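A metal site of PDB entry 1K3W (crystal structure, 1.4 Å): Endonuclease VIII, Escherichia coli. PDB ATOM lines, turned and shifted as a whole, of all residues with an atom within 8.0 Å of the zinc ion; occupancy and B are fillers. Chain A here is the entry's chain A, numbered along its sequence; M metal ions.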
ATOM      1  N   TRP A 176     -32.991  23.691  15.058  1.00  0.00           N
ATOM      2  CA  TRP A 176     -31.857  24.553  15.375  1.00  0.00           C
ATOM      3  C   TRP A 176     -32.026  25.910  14.702  1.00  0.00           C
ATOM      4  O   TRP A 176     -31.757  26.961  15.337  1.00  0.00           O
ATOM      5  CB  TRP A 176     -30.517  23.911  14.967  1.00  0.00           C
ATOM      6  CG  TRP A 176     -29.319  24.790  15.244  1.00  0.00           C
ATOM      7  CD1 TRP A 176     -28.581  24.795  16.399  1.00  0.00           C
ATOM      8  CD2 TRP A 176     -28.721  25.770  14.410  1.00  0.00           C
ATOM      9  NE1 TRP A 176     -27.562  25.735  16.302  1.00  0.00           N
ATOM     10  CE2 TRP A 176     -27.643  26.334  15.093  1.00  0.00           C
ATOM     11  CE3 TRP A 176     -28.986  26.259  13.119  1.00  0.00           C
ATOM     12  CZ2 TRP A 176     -26.832  27.343  14.542  1.00  0.00           C
ATOM     13  CZ3 TRP A 176     -28.195  27.260  12.569  1.00  0.00           C
ATOM     14  CH2 TRP A 176     -27.108  27.802  13.296  1.00  0.00           C
ATOM     15  N   LYS A 228     -25.772  22.200  10.353  1.00  0.00           N
ATOM     16  CA  LYS A 228     -25.349  23.057  11.460  1.00  0.00           C
ATOM     17  C   LYS A 228     -25.211  22.301  12.763  1.00  0.00           C
ATOM     18  O   LYS A 228     -24.353  22.659  13.598  1.00  0.00           O
ATOM     19  CB  LYS A 228     -26.379  24.199  11.635  1.00  0.00           C
ATOM     20  CG  LYS A 228     -26.740  24.960  10.373  1.00  0.00           C
ATOM     21  CD  LYS A 228     -25.633  25.909   9.989  1.00  0.00           C
ATOM     22  CE  LYS A 228     -25.916  26.577   8.653  1.00  0.00           C
ATOM     23  NZ  LYS A 228     -26.918  27.685   8.782  1.00  0.00           N
ATOM     24  N   VAL A 229     -26.030  21.280  12.979  1.00  0.00           N
ATOM     25  CA  VAL A 229     -25.867  20.450  14.172  1.00  0.00           C
ATOM     26  C   VAL A 229     -25.922  18.944  13.914  1.00  0.00           C
ATOM     27  O   VAL A 229     -25.327  18.183  14.715  1.00  0.00           O
ATOM     28  CB  VAL A 229     -26.884  20.776  15.295  1.00  0.00           C
ATOM     29  CG1 VAL A 229     -26.643  22.180  15.882  1.00  0.00           C
ATOM     30  CG2 VAL A 229     -28.328  20.634  14.843  1.00  0.00           C
ATOM     31  N   PRO A 236     -18.154  23.041  18.422  1.00  0.00           N
ATOM     32  CA  PRO A 236     -18.817  24.301  18.811  1.00  0.00           C
ATOM     33  C   PRO A 236     -19.890  24.706  17.794  1.00  0.00           C
ATOM     34  O   PRO A 236     -19.723  24.686  16.578  1.00  0.00           O
ATOM     35  CB  PRO A 236     -17.709  25.355  18.829  1.00  0.00           C
ATOM     36  CG  PRO A 236     -16.500  24.700  18.263  1.00  0.00           C
ATOM     37  CD  PRO A 236     -16.759  23.254  17.978  1.00  0.00           C
ATOM     38  N   CYS A 237     -21.031  25.088  18.337  1.00  0.00           N
ATOM     39  CA  CYS A 237     -22.106  25.704  17.549  1.00  0.00           C
ATOM     40  C   CYS A 237     -21.641  26.947  16.770  1.00  0.00           C
ATOM     41  O   CYS A 237     -20.978  27.765  17.431  1.00  0.00           O
ATOM     42  CB  CYS A 237     -23.209  26.103  18.511  1.00  0.00           C
ATOM     43  SG  CYS A 237     -24.610  26.984  17.755  1.00  0.00           S
ATOM     44  N   GLU A 238     -22.006  27.052  15.484  1.00  0.00           N
ATOM     45  CA  GLU A 238     -21.529  28.195  14.699  1.00  0.00           C
ATOM     46  C   GLU A 238     -22.222  29.513  15.100  1.00  0.00           C
ATOM     47  O   GLU A 238     -21.730  30.596  14.782  1.00  0.00           O
ATOM     48  CB  GLU A 238     -21.713  28.054  13.207  1.00  0.00           C
ATOM     49  CG  GLU A 238     -22.910  27.372  12.618  1.00  0.00           C
ATOM     50  CD  GLU A 238     -22.668  27.288  11.105  1.00  0.00           C
ATOM     51  OE1 GLU A 238     -23.083  28.243  10.426  1.00  0.00           O
ATOM     52  OE2 GLU A 238     -22.052  26.309  10.625  1.00  0.00           O
ATOM     53  N   ARG A 239     -23.367  29.418  15.785  1.00  0.00           N
ATOM     54  CA  ARG A 239     -24.100  30.625  16.209  1.00  0.00           C
ATOM     55  C   ARG A 239     -23.624  31.139  17.568  1.00  0.00           C
ATOM     56  O   ARG A 239     -23.369  32.354  17.731  1.00  0.00           O
ATOM     57  CB  ARG A 239     -25.602  30.294  16.222  1.00  0.00           C
ATOM     58  CG  ARG A 239     -26.455  31.462  16.721  1.00  0.00           C
ATOM     59  CD  ARG A 239     -27.867  31.339  16.112  1.00  0.00           C
ATOM     60  NE  ARG A 239     -28.517  30.163  16.590  1.00  0.00           N
ATOM     61  CZ  ARG A 239     -29.521  29.503  16.037  1.00  0.00           C
ATOM     62  NH1 ARG A 239     -30.098  29.845  14.880  1.00  0.00           N
ATOM     63  NH2 ARG A 239     -29.921  28.451  16.724  1.00  0.00           N
ATOM     64  N   CYS A 240     -23.522  30.270  18.585  1.00  0.00           N
ATOM     65  CA  CYS A 240     -23.180  30.750  19.946  1.00  0.00           C
ATOM     66  C   CYS A 240     -21.944  30.125  20.558  1.00  0.00           C
ATOM     67  O   CYS A 240     -21.571  30.560  21.664  1.00  0.00           O
ATOM     68  CB  CYS A 240     -24.377  30.471  20.871  1.00  0.00           C
ATOM     69  SG  CYS A 240     -24.612  28.753  21.332  1.00  0.00           S
ATOM     70  N   GLY A 241     -21.341  29.121  19.934  1.00  0.00           N
ATOM     71  CA  GLY A 241     -20.112  28.570  20.458  1.00  0.00           C
ATOM     72  C   GLY A 241     -20.241  27.471  21.482  1.00  0.00           C
ATOM     73  O   GLY A 241     -19.229  26.844  21.870  1.00  0.00           O
ATOM     74  N   SER A 242     -21.475  27.207  21.922  1.00  0.00           N
ATOM     75  CA  SER A 242     -21.675  26.092  22.841  1.00  0.00           C
ATOM     76  C   SER A 242     -21.394  24.755  22.136  1.00  0.00           C
ATOM     77  O   SER A 242     -21.487  24.688  20.910  1.00  0.00           O
ATOM     78  CB  SER A 242     -23.071  26.081  23.486  1.00  0.00           C
ATOM     79  OG  SER A 242     -23.194  27.179  24.413  1.00  0.00           O
ATOM     80  N   ILE A 243     -21.034  23.743  22.924  1.00  0.00           N
ATOM     81  CA  ILE A 243     -20.758  22.401  22.377  1.00  0.00           C
ATOM     82  C   ILE A 243     -22.063  21.671  22.140  1.00  0.00           C
ATOM     83  O   ILE A 243     -22.917  21.476  22.995  1.00  0.00           O
ATOM     84  CB  ILE A 243     -19.788  21.587  23.273  1.00  0.00           C
ATOM     85  CG1 ILE A 243     -18.430  22.261  23.505  1.00  0.00           C
ATOM     86  CG2 ILE A 243     -19.542  20.162  22.772  1.00  0.00           C
ATOM     87  CD1 ILE A 243     -17.863  23.108  22.397  1.00  0.00           C
ATOM     88  N   ILE A 244     -22.204  21.295  20.876  1.00  0.00           N
ATOM     89  CA  ILE A 244     -23.393  20.578  20.392  1.00  0.00           C
ATOM     90  C   ILE A 244     -23.460  19.219  21.071  1.00  0.00           C
ATOM     91  O   ILE A 244     -22.417  18.554  21.241  1.00  0.00           O
ATOM     92  CB  ILE A 244     -23.380  20.493  18.850  1.00  0.00           C
ATOM     93  CG1 ILE A 244     -23.538  21.910  18.249  1.00  0.00           C
ATOM     94  CG2 ILE A 244     -24.407  19.523  18.275  1.00  0.00           C
ATOM     95  CD1 ILE A 244     -23.022  22.071  16.840  1.00  0.00           C
ATOM     96  N   TRP A 256     -28.441  18.873  19.013  1.00  0.00           N
ATOM     97  CA  TRP A 256     -28.952  20.215  19.317  1.00  0.00           C
ATOM     98  C   TRP A 256     -27.906  21.013  20.087  1.00  0.00           C
ATOM     99  O   TRP A 256     -26.973  20.442  20.645  1.00  0.00           O
ATOM    100  CB  TRP A 256     -30.232  20.092  20.154  1.00  0.00           C
ATOM    101  CG  TRP A 256     -29.968  19.497  21.519  1.00  0.00           C
ATOM    102  CD1 TRP A 256     -29.546  18.237  21.854  1.00  0.00           C
ATOM    103  CD2 TRP A 256     -30.135  20.198  22.739  1.00  0.00           C
ATOM    104  NE1 TRP A 256     -29.451  18.104  23.220  1.00  0.00           N
ATOM    105  CE2 TRP A 256     -29.805  19.317  23.778  1.00  0.00           C
ATOM    106  CE3 TRP A 256     -30.554  21.492  23.021  1.00  0.00           C
ATOM    107  CZ2 TRP A 256     -29.862  19.661  25.128  1.00  0.00           C
ATOM    108  CZ3 TRP A 256     -30.601  21.858  24.357  1.00  0.00           C
ATOM    109  CH2 TRP A 256     -30.266  20.975  25.383  1.00  0.00           C
ATOM    110  N   CYS A 257     -28.117  22.318  20.148  1.00  0.00           N
ATOM    111  CA  CYS A 257     -27.224  23.187  20.930  1.00  0.00           C
ATOM    112  C   CYS A 257     -27.885  23.719  22.199  1.00  0.00           C
ATOM    113  O   CYS A 257     -28.933  24.422  22.129  1.00  0.00           O
ATOM    114  CB  CYS A 257     -26.796  24.388  20.060  1.00  0.00           C
ATOM    115  SG  CYS A 257     -25.682  25.446  21.033  1.00  0.00           S
ATOM    116  N   PRO A 258     -27.245  23.454  23.369  1.00  0.00           N
ATOM    117  CA  PRO A 258     -27.823  23.928  24.637  1.00  0.00           C
ATOM    118  C   PRO A 258     -27.709  25.434  24.825  1.00  0.00           C
ATOM    119  O   PRO A 258     -28.376  25.997  25.703  1.00  0.00           O
ATOM    120  CB  PRO A 258     -26.965  23.211  25.685  1.00  0.00           C
ATOM    121  CG  PRO A 258     -25.647  23.069  24.971  1.00  0.00           C
ATOM    122  CD  PRO A 258     -26.001  22.671  23.572  1.00  0.00           C
ATOM    123  N   GLY A 259     -26.911  26.111  24.003  1.00  0.00           N
ATOM    124  CA  GLY A 259     -26.744  27.575  24.193  1.00  0.00           C
ATOM    125  C   GLY A 259     -27.792  28.389  23.450  1.00  0.00           C
ATOM    126  O   GLY A 259     -28.092  29.548  23.822  1.00  0.00           O
ATOM    127  N   CYS A 260     -28.386  27.856  22.369  1.00  0.00           N
ATOM    128  CA  CYS A 260     -29.261  28.722  21.568  1.00  0.00           C
ATOM    129  C   CYS A 260     -30.534  27.993  21.131  1.00  0.00           C
ATOM    130  O   CYS A 260     -31.269  28.543  20.292  1.00  0.00           O
ATOM    131  CB  CYS A 260     -28.499  29.286  20.346  1.00  0.00           C
ATOM    132  SG  CYS A 260     -27.915  27.995  19.177  1.00  0.00           S
ATOM    133  N   GLN A 261     -30.834  26.796  21.623  1.00  0.00           N
ATOM    134  CA  GLN A 261     -32.139  26.147  21.415  1.00  0.00           C
ATOM    135  C   GLN A 261     -32.846  26.052  22.785  1.00  0.00           C
ATOM    136  O   GLN A 261     -32.214  25.553  23.740  1.00  0.00           O
ATOM    137  CB  GLN A 261     -32.022  24.760  20.779  1.00  0.00           C
ATOM    138  CG  GLN A 261     -31.566  24.896  19.314  1.00  0.00           C
ATOM    139  CD  GLN A 261     -31.397  23.502  18.721  1.00  0.00           C
ATOM    140  OE1 GLN A 261     -30.244  23.058  18.553  1.00  0.00           O
ATOM    141  NE2 GLN A 261     -32.503  22.796  18.371  1.00  0.00           N
ATOM    142  N   HIS A 262     -34.078  26.539  22.820  1.00  0.00           N
ATOM    143  CA  HIS A 262     -34.875  26.661  24.056  1.00  0.00           C
ATOM    144  C   HIS A 262     -36.352  26.304  23.892  1.00  0.00           C
ATOM    145  O   HIS A 262     -36.730  26.140  22.727  1.00  0.00           O
ATOM    146  CB  HIS A 262     -34.889  28.108  24.607  1.00  0.00           C
ATOM    147  CG  HIS A 262     -33.482  28.607  24.742  1.00  0.00           C
ATOM    148  ND1 HIS A 262     -32.648  28.328  25.794  1.00  0.00           N
ATOM    149  CD2 HIS A 262     -32.739  29.367  23.882  1.00  0.00           C
ATOM    150  CE1 HIS A 262     -31.494  28.903  25.580  1.00  0.00           C
ATOM    151  NE2 HIS A 262     -31.509  29.535  24.428  1.00  0.00           N
ATOM    152  OXT HIS A 262     -37.060  26.282  24.913  1.00  0.00           O
HETATM  153 ZN    ZN M   1     -25.741  27.435  19.804  1.00  0.00          ZN
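The nearest printed residue that does not touch the zinc ion is Gly 259 (4.3 Å).
SG of Cys 240 binds the zinc ion (2.3 Å).
The side-chain sulfur (SG) of Cys 260 is bound to the zinc ion, at 2.3 Å.
SG of Cys 257 binds the zinc ion, at 2.3 Å.
The zinc ion is bound by the side-chain sulfur (SG) of Cys 237 (2.4 Å).
The zinc ion has four donor atoms within binding distance.
SG of Cys 240 sits close to N of Ser 242 (3.5 Å).
N of Cys 237 sits at hydrogen-bond distance from O of Ser 242.
The guanidinium group (NH2) of Arg 239 lies close to the side-chain sulfur (SG) of Cys 260, 3.2 Å away.
SG of Cys 260 lies close to NE1 of Trp 176 (3.7 Å).
The side-chain amide oxygen (OE1) of Gln 261 is in hydrogen-bond range of the backbone NH (N) of Cys 257, at 2.8 Å.
N of Arg 239 sits close to SG of Cys 237, 3.4 Å away.
The indole nitrogen (NE1) of Trp 176 lies close to the side-chain sulfur (SG) of Cys 237.
N of Gly 259 lies close to SG of Cys 257, at 3.3 Å.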
